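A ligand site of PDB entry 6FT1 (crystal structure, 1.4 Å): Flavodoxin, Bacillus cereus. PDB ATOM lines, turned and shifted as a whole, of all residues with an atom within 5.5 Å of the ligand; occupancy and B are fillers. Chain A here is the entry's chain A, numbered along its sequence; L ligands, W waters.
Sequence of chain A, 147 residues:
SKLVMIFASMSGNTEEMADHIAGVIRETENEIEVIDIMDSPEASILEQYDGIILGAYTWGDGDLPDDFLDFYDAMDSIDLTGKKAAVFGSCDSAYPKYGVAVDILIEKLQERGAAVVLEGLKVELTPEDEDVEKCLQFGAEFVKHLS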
ATOM      1  N   ALA A   8       7.098  -4.484 -11.774  1.00  0.00           N
ATOM      2  CA  ALA A   8       7.277  -3.673 -12.971  1.00  0.00           C
ATOM      3  C   ALA A   8       8.701  -3.849 -13.468  1.00  0.00           C
ATOM      4  O   ALA A   8       9.669  -3.743 -12.697  1.00  0.00           O
ATOM      5  CB  ALA A   8       6.923  -2.201 -12.648  1.00  0.00           C
ATOM      6  N   SER A   9       8.896  -4.096 -14.766  1.00  0.00           N
ATOM      7  CA  SER A   9      10.241  -4.211 -15.313  1.00  0.00           C
ATOM      8  C   SER A   9      10.203  -3.829 -16.800  1.00  0.00           C
ATOM      9  O   SER A   9       9.381  -4.354 -17.568  1.00  0.00           O
ATOM     10  CB  SER A   9      10.811  -5.633 -15.168  1.00  0.00           C
ATOM     11  OG  SER A   9      12.189  -5.707 -15.490  1.00  0.00           O
ATOM     12  N   MET A  10      11.031  -2.885 -17.146  1.00  0.00           N
ATOM     13  CA  MET A  10      11.155  -2.461 -18.546  1.00  0.00           C
ATOM     14  C   MET A  10      12.328  -3.148 -19.227  1.00  0.00           C
ATOM     15  O   MET A  10      12.123  -3.725 -20.300  1.00  0.00           O
ATOM     16  CB  MET A  10      11.263  -0.946 -18.707  1.00  0.00           C
ATOM     17  CG  MET A  10      11.286  -0.427 -20.172  1.00  0.00           C
ATOM     18  SD  MET A  10      11.552   1.362 -20.140  1.00  0.00           S
ATOM     19  CE  MET A  10       9.995   2.026 -19.539  1.00  0.00           C
ATOM     20  N   SER A  11      13.498  -3.212 -18.603  1.00  0.00           N
ATOM     21  CA  SER A  11      14.685  -3.820 -19.206  1.00  0.00           C
ATOM     22  C   SER A  11      15.055  -5.175 -18.619  1.00  0.00           C
ATOM     23  O   SER A  11      16.155  -5.661 -18.886  1.00  0.00           O
ATOM     24  CB  SER A  11      15.890  -2.884 -19.119  1.00  0.00           C
ATOM     25  OG  SER A  11      16.600  -2.981 -17.899  1.00  0.00           O
ATOM     26  N   GLY A  12      14.167  -5.752 -17.815  1.00  0.00           N
ATOM     27  CA  GLY A  12      14.317  -7.094 -17.324  1.00  0.00           C
ATOM     28  C   GLY A  12      14.951  -7.264 -15.947  1.00  0.00           C
ATOM     29  O   GLY A  12      14.921  -8.414 -15.433  1.00  0.00           O
ATOM     30  N   ASN A  13      15.598  -6.230 -15.368  1.00  0.00           N
ATOM     31  CA  ASN A  13      16.356  -6.454 -14.129  1.00  0.00           C
ATOM     32  C   ASN A  13      15.431  -6.741 -12.949  1.00  0.00           C
ATOM     33  O   ASN A  13      15.634  -7.693 -12.174  1.00  0.00           O
ATOM     34  CB  ASN A  13      17.151  -5.177 -13.874  1.00  0.00           C
ATOM     35  CG  ASN A  13      18.243  -4.916 -14.929  1.00  0.00           C
ATOM     36  OD1 ASN A  13      18.812  -5.881 -15.458  1.00  0.00           O
ATOM     37  ND2 ASN A  13      18.561  -3.606 -15.261  1.00  0.00           N
ATOM     38  N   THR A  14      14.375  -5.912 -12.794  1.00  0.00           N
ATOM     39  CA  THR A  14      13.444  -6.174 -11.716  1.00  0.00           C
ATOM     40  C   THR A  14      12.704  -7.472 -11.974  1.00  0.00           C
ATOM     41  O   THR A  14      12.383  -8.171 -11.040  1.00  0.00           O
ATOM     42  CB  THR A  14      12.471  -5.003 -11.561  1.00  0.00           C
ATOM     43  OG1 THR A  14      13.216  -3.785 -11.413  1.00  0.00           O
ATOM     44  CG2 THR A  14      11.515  -5.171 -10.324  1.00  0.00           C
ATOM     45  N   GLU A  15      12.484  -7.823 -13.259  1.00  0.00           N
ATOM     46  CA  GLU A  15      11.858  -9.102 -13.597  1.00  0.00           C
ATOM     47  C   GLU A  15      12.697 -10.267 -13.104  1.00  0.00           C
ATOM     48  O   GLU A  15      12.156 -11.240 -12.568  1.00  0.00           O
ATOM     49  CB  GLU A  15      11.666  -9.207 -15.111  1.00  0.00           C
ATOM     50  CG  GLU A  15      10.811 -10.415 -15.518  1.00  0.00           C
ATOM     51  CD  GLU A  15      10.678 -10.590 -17.040  1.00  0.00           C
ATOM     52  OE1 GLU A  15      11.402  -9.905 -17.748  1.00  0.00           O
ATOM     53  OE2 GLU A  15       9.903 -11.436 -17.490  1.00  0.00           O
ATOM     54  N   TYR A  57      11.230  -0.857 -10.614  1.00  0.00           N
ATOM     55  CA  TYR A  57      12.345   0.058 -10.909  1.00  0.00           C
ATOM     56  C   TYR A  57      11.947   1.518 -10.620  1.00  0.00           C
ATOM     57  O   TYR A  57      10.757   1.804 -10.420  1.00  0.00           O
ATOM     58  CB  TYR A  57      12.788  -0.048 -12.395  1.00  0.00           C
ATOM     59  CG  TYR A  57      11.702   0.216 -13.416  1.00  0.00           C
ATOM     60  CD1 TYR A  57      10.875  -0.834 -13.864  1.00  0.00           C
ATOM     61  CD2 TYR A  57      11.493   1.534 -13.953  1.00  0.00           C
ATOM     62  CE1 TYR A  57       9.848  -0.588 -14.741  1.00  0.00           C
ATOM     63  CE2 TYR A  57      10.525   1.730 -14.917  1.00  0.00           C
ATOM     64  CZ  TYR A  57       9.730   0.686 -15.277  1.00  0.00           C
ATOM     65  OH  TYR A  57       8.707   0.892 -16.208  1.00  0.00           O
ATOM     66  N   THR A  58      12.904   2.422 -10.610  1.00  0.00           N
ATOM     67  CA  THR A  58      12.612   3.843 -10.410  1.00  0.00           C
ATOM     68  C   THR A  58      12.756   4.527 -11.761  1.00  0.00           C
ATOM     69  O   THR A  58      13.661   4.208 -12.546  1.00  0.00           O
ATOM     70  CB  THR A  58      13.620   4.441  -9.391  1.00  0.00           C
ATOM     71  OG1 THR A  58      13.451   3.715  -8.175  1.00  0.00           O
ATOM     72  CG2 THR A  58      13.287   5.917  -9.055  1.00  0.00           C
ATOM     73  N   TRP A  59      11.863   5.452 -12.017  1.00  0.00           N
ATOM     74  CA  TRP A  59      11.891   6.180 -13.267  1.00  0.00           C
ATOM     75  C   TRP A  59      12.115   7.651 -12.996  1.00  0.00           C
ATOM     76  O   TRP A  59      12.546   8.025 -11.892  1.00  0.00           O
ATOM     77  CB  TRP A  59      10.563   5.928 -13.950  1.00  0.00           C
ATOM     78  CG  TRP A  59      10.491   6.300 -15.396  1.00  0.00           C
ATOM     79  CD1 TRP A  59       9.717   7.270 -15.955  1.00  0.00           C
ATOM     80  CD2 TRP A  59      11.183   5.645 -16.452  1.00  0.00           C
ATOM     81  NE1 TRP A  59       9.938   7.291 -17.326  1.00  0.00           N
ATOM     82  CE2 TRP A  59      10.818   6.290 -17.638  1.00  0.00           C
ATOM     83  CE3 TRP A  59      12.125   4.610 -16.497  1.00  0.00           C
ATOM     84  CZ2 TRP A  59      11.343   5.922 -18.877  1.00  0.00           C
ATOM     85  CZ3 TRP A  59      12.614   4.215 -17.734  1.00  0.00           C
ATOM     86  CH2 TRP A  59      12.231   4.885 -18.899  1.00  0.00           C
ATOM     87  N   GLY A  60      11.793   8.469 -13.990  1.00  0.00           N
ATOM     88  CA  GLY A  60      12.256   9.845 -14.075  1.00  0.00           C
ATOM     89  C   GLY A  60      12.020  10.676 -12.845  1.00  0.00           C
ATOM     90  O   GLY A  60      10.899  10.744 -12.353  1.00  0.00           O
ATOM     91  N   ASP A  61      13.087  11.356 -12.373  1.00  0.00           N
ATOM     92  CA  ASP A  61      13.038  12.237 -11.210  1.00  0.00           C
ATOM     93  C   ASP A  61      12.577  11.517  -9.939  1.00  0.00           C
ATOM     94  O   ASP A  61      11.833  12.065  -9.119  1.00  0.00           O
ATOM     95  CB  ASP A  61      12.234  13.495 -11.466  1.00  0.00           C
ATOM     96  CG  ASP A  61      12.765  14.683 -10.677  1.00  0.00           C
ATOM     97  OD1 ASP A  61      13.970  14.643 -10.276  1.00  0.00           O
ATOM     98  OD2 ASP A  61      11.990  15.633 -10.449  1.00  0.00           O
ATOM     99  N   GLY A  62      13.037  10.278  -9.764  1.00  0.00           N
ATOM    100  CA  GLY A  62      12.694   9.504  -8.580  1.00  0.00           C
ATOM    101  C   GLY A  62      11.212   9.174  -8.527  1.00  0.00           C
ATOM    102  O   GLY A  62      10.554   9.398  -7.496  1.00  0.00           O
ATOM    103  N   ASP A  63      10.654   8.702  -9.628  1.00  0.00           N
ATOM    104  CA  ASP A  63       9.220   8.390  -9.649  1.00  0.00           C
ATOM    105  C   ASP A  63       8.998   6.881  -9.778  1.00  0.00           C
ATOM    106  O   ASP A  63       9.889   6.088 -10.144  1.00  0.00           O
ATOM    107  CB  ASP A  63       8.563   9.074 -10.863  1.00  0.00           C
ATOM    108  CG  ASP A  63       8.445  10.599 -10.733  1.00  0.00           C
ATOM    109  OD1 ASP A  63       8.531  11.137  -9.628  1.00  0.00           O
ATOM    110  OD2 ASP A  63       8.237  11.261 -11.784  1.00  0.00           O
ATOM    111  N   SER A  90      15.156  -3.009  -8.950  1.00  0.00           N
ATOM    112  CA  SER A  90      16.434  -2.620  -9.522  1.00  0.00           C
ATOM    113  C   SER A  90      16.504  -1.095  -9.647  1.00  0.00           C
ATOM    114  O   SER A  90      15.488  -0.396  -9.782  1.00  0.00           O
ATOM    115  CB  SER A  90      16.595  -3.267 -10.910  1.00  0.00           C
ATOM    116  OG  SER A  90      17.872  -2.952 -11.438  1.00  0.00           O
ATOM    117  N   CYS A  91      17.738  -0.595  -9.616  1.00  0.00           N
ATOM    118  CA  CYS A  91      18.038   0.808  -9.327  1.00  0.00           C
ATOM    119  C   CYS A  91      19.243   1.235 -10.161  1.00  0.00           C
ATOM    120  O   CYS A  91      19.907   0.389 -10.756  1.00  0.00           O
ATOM    121  CB  CYS A  91      18.380   0.963  -7.852  1.00  0.00           C
ATOM    122  SG  CYS A  91      17.187   0.277  -6.709  1.00  0.00           S
ATOM    123  N   ASP A  92      19.584   2.535 -10.173  1.00  0.00           N
ATOM    124  CA  ASP A  92      20.815   2.968 -10.846  1.00  0.00           C
ATOM    125  C   ASP A  92      21.435   4.156 -10.131  1.00  0.00           C
ATOM    126  O   ASP A  92      20.811   5.224 -10.051  1.00  0.00           O
ATOM    127  CB  ASP A  92      20.473   3.308 -12.301  1.00  0.00           C
ATOM    128  CG  ASP A  92      21.656   3.666 -13.155  1.00  0.00           C
ATOM    129  OD1 ASP A  92      22.786   3.814 -12.670  1.00  0.00           O
ATOM    130  OD2 ASP A  92      21.362   3.754 -14.401  1.00  0.00           O
ATOM    131  N   SER A  93      22.672   3.980  -9.665  1.00  0.00           N
ATOM    132  CA  SER A  93      23.358   5.009  -8.879  1.00  0.00           C
ATOM    133  C   SER A  93      23.930   6.148  -9.740  1.00  0.00           C
ATOM    134  O   SER A  93      24.654   7.011  -9.205  1.00  0.00           O
ATOM    135  CB  SER A  93      24.411   4.358  -7.954  1.00  0.00           C
ATOM    136  OG  SER A  93      25.471   3.840  -8.760  1.00  0.00           O
ATOM    137  N   TYR A  95      21.726   8.101 -10.823  1.00  0.00           N
ATOM    138  CA  TYR A  95      20.610   8.948 -10.475  1.00  0.00           C
ATOM    139  C   TYR A  95      20.689   9.293  -8.998  1.00  0.00           C
ATOM    140  O   TYR A  95      21.040   8.433  -8.185  1.00  0.00           O
ATOM    141  CB  TYR A  95      19.278   8.255 -10.734  1.00  0.00           C
ATOM    142  CG  TYR A  95      19.062   8.094 -12.238  1.00  0.00           C
ATOM    143  CD1 TYR A  95      19.587   6.971 -12.905  1.00  0.00           C
ATOM    144  CD2 TYR A  95      18.407   9.067 -12.965  1.00  0.00           C
ATOM    145  CE1 TYR A  95      19.425   6.835 -14.290  1.00  0.00           C
ATOM    146  CE2 TYR A  95      18.223   8.913 -14.358  1.00  0.00           C
ATOM    147  CZ  TYR A  95      18.748   7.819 -14.978  1.00  0.00           C
ATOM    148  OH  TYR A  95      18.527   7.703 -16.324  1.00  0.00           O
ATOM    149  N   LYS A  97      18.208  10.062  -6.866  1.00  0.00           N
ATOM    150  CA  LYS A  97      17.049   9.510  -6.152  1.00  0.00           C
ATOM    151  C   LYS A  97      17.006   7.994  -6.356  1.00  0.00           C
ATOM    152  O   LYS A  97      16.146   7.431  -7.058  1.00  0.00           O
ATOM    153  CB  LYS A  97      15.773  10.255  -6.543  1.00  0.00           C
ATOM    154  CG  LYS A  97      15.871  11.807  -6.424  1.00  0.00           C
ATOM    155  CD  LYS A  97      14.599  12.489  -6.872  1.00  0.00           C
ATOM    156  CE  LYS A  97      14.741  13.998  -6.755  1.00  0.00           C
ATOM    157  NZ  LYS A  97      13.552  14.688  -7.276  1.00  0.00           N
ATOM    158  N   TYR A  98      17.946   7.350  -5.699  1.00  0.00           N
ATOM    159  CA  TYR A  98      18.316   5.967  -6.030  1.00  0.00           C
ATOM    160  C   TYR A  98      17.283   5.021  -5.455  1.00  0.00           C
ATOM    161  O   TYR A  98      17.091   4.923  -4.239  1.00  0.00           O
ATOM    162  CB  TYR A  98      19.686   5.636  -5.453  1.00  0.00           C
ATOM    163  CG  TYR A  98      20.133   4.214  -5.558  1.00  0.00           C
ATOM    164  CD1 TYR A  98      20.682   3.729  -6.761  1.00  0.00           C
ATOM    165  CD2 TYR A  98      19.988   3.345  -4.491  1.00  0.00           C
ATOM    166  CE1 TYR A  98      21.181   2.464  -6.836  1.00  0.00           C
ATOM    167  CE2 TYR A  98      20.470   2.029  -4.561  1.00  0.00           C
ATOM    168  CZ  TYR A  98      21.037   1.596  -5.747  1.00  0.00           C
ATOM    169  OH  TYR A  98      21.559   0.294  -5.886  1.00  0.00           O
ATOM    170  N   GLY A  99      16.655   4.246  -6.323  1.00  0.00           N
ATOM    171  CA  GLY A  99      15.703   3.251  -5.902  1.00  0.00           C
ATOM    172  C   GLY A  99      14.515   3.769  -5.134  1.00  0.00           C
ATOM    173  O   GLY A  99      13.858   2.995  -4.443  1.00  0.00           O
ATOM    174  N   VAL A 100      14.202   5.051  -5.240  1.00  0.00           N
ATOM    175  CA  VAL A 100      13.131   5.588  -4.390  1.00  0.00           C
ATOM    176  C   VAL A 100      11.741   5.085  -4.736  1.00  0.00           C
ATOM    177  O   VAL A 100      10.834   5.191  -3.910  1.00  0.00           O
ATOM    178  CB  VAL A 100      13.076   7.112  -4.252  1.00  0.00           C
ATOM    179  CG1 VAL A 100      14.337   7.569  -3.518  1.00  0.00           C
ATOM    180  CG2 VAL A 100      12.932   7.790  -5.593  1.00  0.00           C
ATOM    181  N   LEU A 125      21.132  -2.147 -11.129  1.00  0.00           N
ATOM    182  CA  LEU A 125      21.029  -2.606 -12.537  1.00  0.00           C
ATOM    183  C   LEU A 125      20.840  -4.134 -12.579  1.00  0.00           C
ATOM    184  O   LEU A 125      19.922  -4.632 -11.934  1.00  0.00           O
ATOM    185  CB  LEU A 125      22.160  -2.085 -13.377  1.00  0.00           C
ATOM    186  CG  LEU A 125      22.312  -0.525 -13.552  1.00  0.00           C
ATOM    187  CD1 LEU A 125      23.596  -0.110 -14.346  1.00  0.00           C
ATOM    188  CD2 LEU A 125      20.983  -0.061 -14.294  1.00  0.00           C
ATOM    189  N   THR A 126      21.632  -4.883 -13.373  1.00  0.00           N
ATOM    190  CA  THR A 126      21.386  -6.310 -13.513  1.00  0.00           C
ATOM    191  C   THR A 126      21.973  -7.076 -12.340  1.00  0.00           C
ATOM    192  O   THR A 126      23.137  -6.899 -11.997  1.00  0.00           O
ATOM    193  CB  THR A 126      21.998  -6.793 -14.826  1.00  0.00           C
ATOM    194  OG1 THR A 126      21.482  -6.030 -15.924  1.00  0.00           O
ATOM    195  CG2 THR A 126      21.630  -8.260 -15.094  1.00  0.00           C
HETATM  196  N1  LIG L   1      17.071   4.692 -11.264  1.00  0.00           N
HETATM  197  C1  LIG L   1      17.032   5.247  -9.996  1.00  0.00           C
HETATM  198  O1  LIG L   1      17.558   4.603  -9.102  1.00  0.00           O
HETATM  199  N2  LIG L   1      16.598   6.547  -9.778  1.00  0.00           N
HETATM  200  C2  LIG L   1      15.978   7.276 -10.758  1.00  0.00           C
HETATM  201  O2  LIG L   1      15.580   8.421 -10.446  1.00  0.00           O
HETATM  202  C3  LIG L   1      16.000   6.731 -12.058  1.00  0.00           C
HETATM  203  N3  LIG L   1      15.456   7.384 -13.146  1.00  0.00           N
HETATM  204  C4  LIG L   1      15.470   6.761 -14.399  1.00  0.00           C
HETATM  205  C5  LIG L   1      14.939   7.409 -15.513  1.00  0.00           C
HETATM  206  C6  LIG L   1      15.099   6.871 -16.794  1.00  0.00           C
HETATM  207  C7  LIG L   1      14.465   7.667 -17.924  1.00  0.00           C
HETATM  208  C8  LIG L   1      15.633   5.599 -16.985  1.00  0.00           C
HETATM  209  C9  LIG L   1      15.817   4.997 -18.355  1.00  0.00           C
HETATM  210  C10 LIG L   1      16.156   4.932 -15.860  1.00  0.00           C
HETATM  211  C11 LIG L   1      15.945   5.458 -14.564  1.00  0.00           C
HETATM  212  N4  LIG L   1      16.542   4.856 -13.508  1.00  0.00           N
HETATM  213  C12 LIG L   1      16.498   5.432 -12.247  1.00  0.00           C
HETATM  214  C13 LIG L   1      17.209   3.485 -13.693  1.00  0.00           C
HETATM  215  C14 LIG L   1      16.315   2.233 -13.764  1.00  0.00           C
HETATM  216  O3  LIG L   1      15.611   2.080 -12.560  1.00  0.00           O
HETATM  217  C15 LIG L   1      17.283   1.035 -13.894  1.00  0.00           C
HETATM  218  O4  LIG L   1      17.861   1.044 -15.217  1.00  0.00           O
HETATM  219  C16 LIG L   1      16.654  -0.324 -13.547  1.00  0.00           C
HETATM  220  O5  LIG L   1      17.651  -1.308 -13.661  1.00  0.00           O
HETATM  221  C17 LIG L   1      15.514  -0.690 -14.499  1.00  0.00           C
HETATM  222  O6  LIG L   1      14.890  -1.842 -13.959  1.00  0.00           O
HETATM  223  P1  LIG L   1      14.211  -2.759 -15.037  1.00  0.00           P
HETATM  224  O7  LIG L   1      13.379  -3.659 -14.220  1.00  0.00           O
HETATM  225  O8  LIG L   1      15.279  -3.497 -15.816  1.00  0.00           O
HETATM  226  O9  LIG L   1      13.328  -1.949 -15.926  1.00  0.00           O
HETATM  227  O   HOH W   1      17.103  10.727  -9.506  1.00  0.00           O
HETATM  228  O   HOH W   2      19.073   5.440 -17.583  1.00  0.00           O
HETATM  229  O   HOH W   3      13.543   0.692 -16.695  1.00  0.00           O
HETATM  230  O   HOH W   4      11.697   9.688 -17.292  1.00  0.00           O
HETATM  231  O   HOH W   5      17.988  -0.777 -17.265  1.00  0.00           O
HETATM  232  O   HOH W   6      19.242   2.746 -16.749  1.00  0.00           O
HETATM  233  O   HOH W   7      15.413  10.850 -15.859  1.00  0.00           O
HETATM  234  O   HOH W   8      15.691  10.492 -13.090  1.00  0.00           O
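The side-chain hydroxyl (OG1) of Thr 126 is in hydrogen-bond range of the side-chain amide oxygen (OD1) of Asn 13, 2.7 Å away.
The backbone NH (N) of Leu 125 lies within hydrogen-bond range of the backbone carbonyl oxygen (O) of Cys 91 (2.8 Å).
The side-chain hydroxyl (OG) of Ser 9 lies within hydrogen-bond range of the backbone NH (N) of Thr 14 (3.5 Å).
The side-chain hydroxyl (OG) of Ser 90 is in hydrogen-bond range of the backbone carbonyl oxygen (O) of Leu 125, 2.7 Å away.
NZ of Lys 97 lies within salt-bridge range of OD1 of Asp 61, 3.0 Å away.
The side-chain hydroxyl of Thr 14 is in hydrogen-bond range of the backbone NH of Ser 90.
N of Gly 12 is in hydrogen-bond range of OG of Ser 9, at 3.1 Å.
OG of Ser 9 lies within hydrogen-bond range of N of Glu 15, at 3.1 Å.
Water W6 bridges an oxygen (O4) of the ligand (2.7 Å) and the side-chain carboxylate of Asp 92 (3.3 Å).
Water W5 bridges OG of Ser 11 (2.7 Å) and O4 of the ligand (2.7 Å).
Water W1 bridges O2 of the ligand (2.9 Å) and N of Lys 97 (2.9 Å).
Water W8 lies within hydrogen-bond range of N of Asp 61 (2.8 Å) and N3 of the ligand (3.1 Å).
N of Asp 92 sits at hydrogen-bond distance from O1 of the ligand (3.1 Å).
ND2 of Asn 13 lies within hydrogen-bond range of O5 of the ligand (2.9 Å).
O of Thr 58 is in hydrogen-bond range of O3 of the ligand (2.9 Å).
O8 of the ligand lies within hydrogen-bond range of N of Asn 13, 2.8 Å away.
O8 of the ligand lies within hydrogen-bond range of N of Gly 12, 3.2 Å away.
OG of Ser 11 is in hydrogen-bond range of O8 of the ligand (2.5 Å).
An oxygen (O5) of the ligand sits at hydrogen-bond distance from the side-chain hydroxyl of Ser 90, 2.8 Å away.
An oxygen (O7) of the ligand sits at hydrogen-bond distance from the side-chain hydroxyl of Ser 9 (2.7 Å).
The backbone NH of Thr 14 sits at hydrogen-bond distance from an oxygen (O7) of the ligand, at 2.8 Å.
N of Gly 99 sits at hydrogen-bond distance from O1 of the ligand.
The backbone NH of Met 10 is in hydrogen-bond range of an oxygen (O9) of the ligand, at 2.8 Å.
The backbone carbonyl oxygen (O) of Lys 97 sits at hydrogen-bond distance from a nitrogen (N2) of the ligand (2.9 Å).
O9 of the ligand is in hydrogen-bond range of N of Ser 11 (3.0 Å).
O7 of the ligand sits at hydrogen-bond distance from OG1 of Thr 14, 2.8 Å away.
An oxygen (O3) of the ligand lies within hydrogen-bond range of the backbone NH (N) of Thr 58, 3.4 Å away.
The backbone NH (N) of Gly 62 is in hydrogen-bond range of an oxygen (O2) of the ligand (3.2 Å).
O of Trp 59 lies close to N3 of the ligand, 3.2 Å away.
Tyr 57 touches the ligand (CB to O6, 3.2 Å).
Gly 60 touches the ligand (N to C5, 3.7 Å).
Cys 91 touches the ligand.
Tyr 95 touches the ligand (CB to N2, 3.3 Å).
CA of Tyr 98 touches O1 of the ligand, 3.4 Å away.
Leu 125 touches the ligand.
Hydrophobic or aromatic side chains within 4 Å of the ligand: Met 10, Tyr 57, Trp 59, Tyr 95 and Leu 125.
Of the 26 residues printed, 19 come within 4 Å of the ligand.
The nearest printed residue that does not touch the ligand is Ala 8 (4.01 Å).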
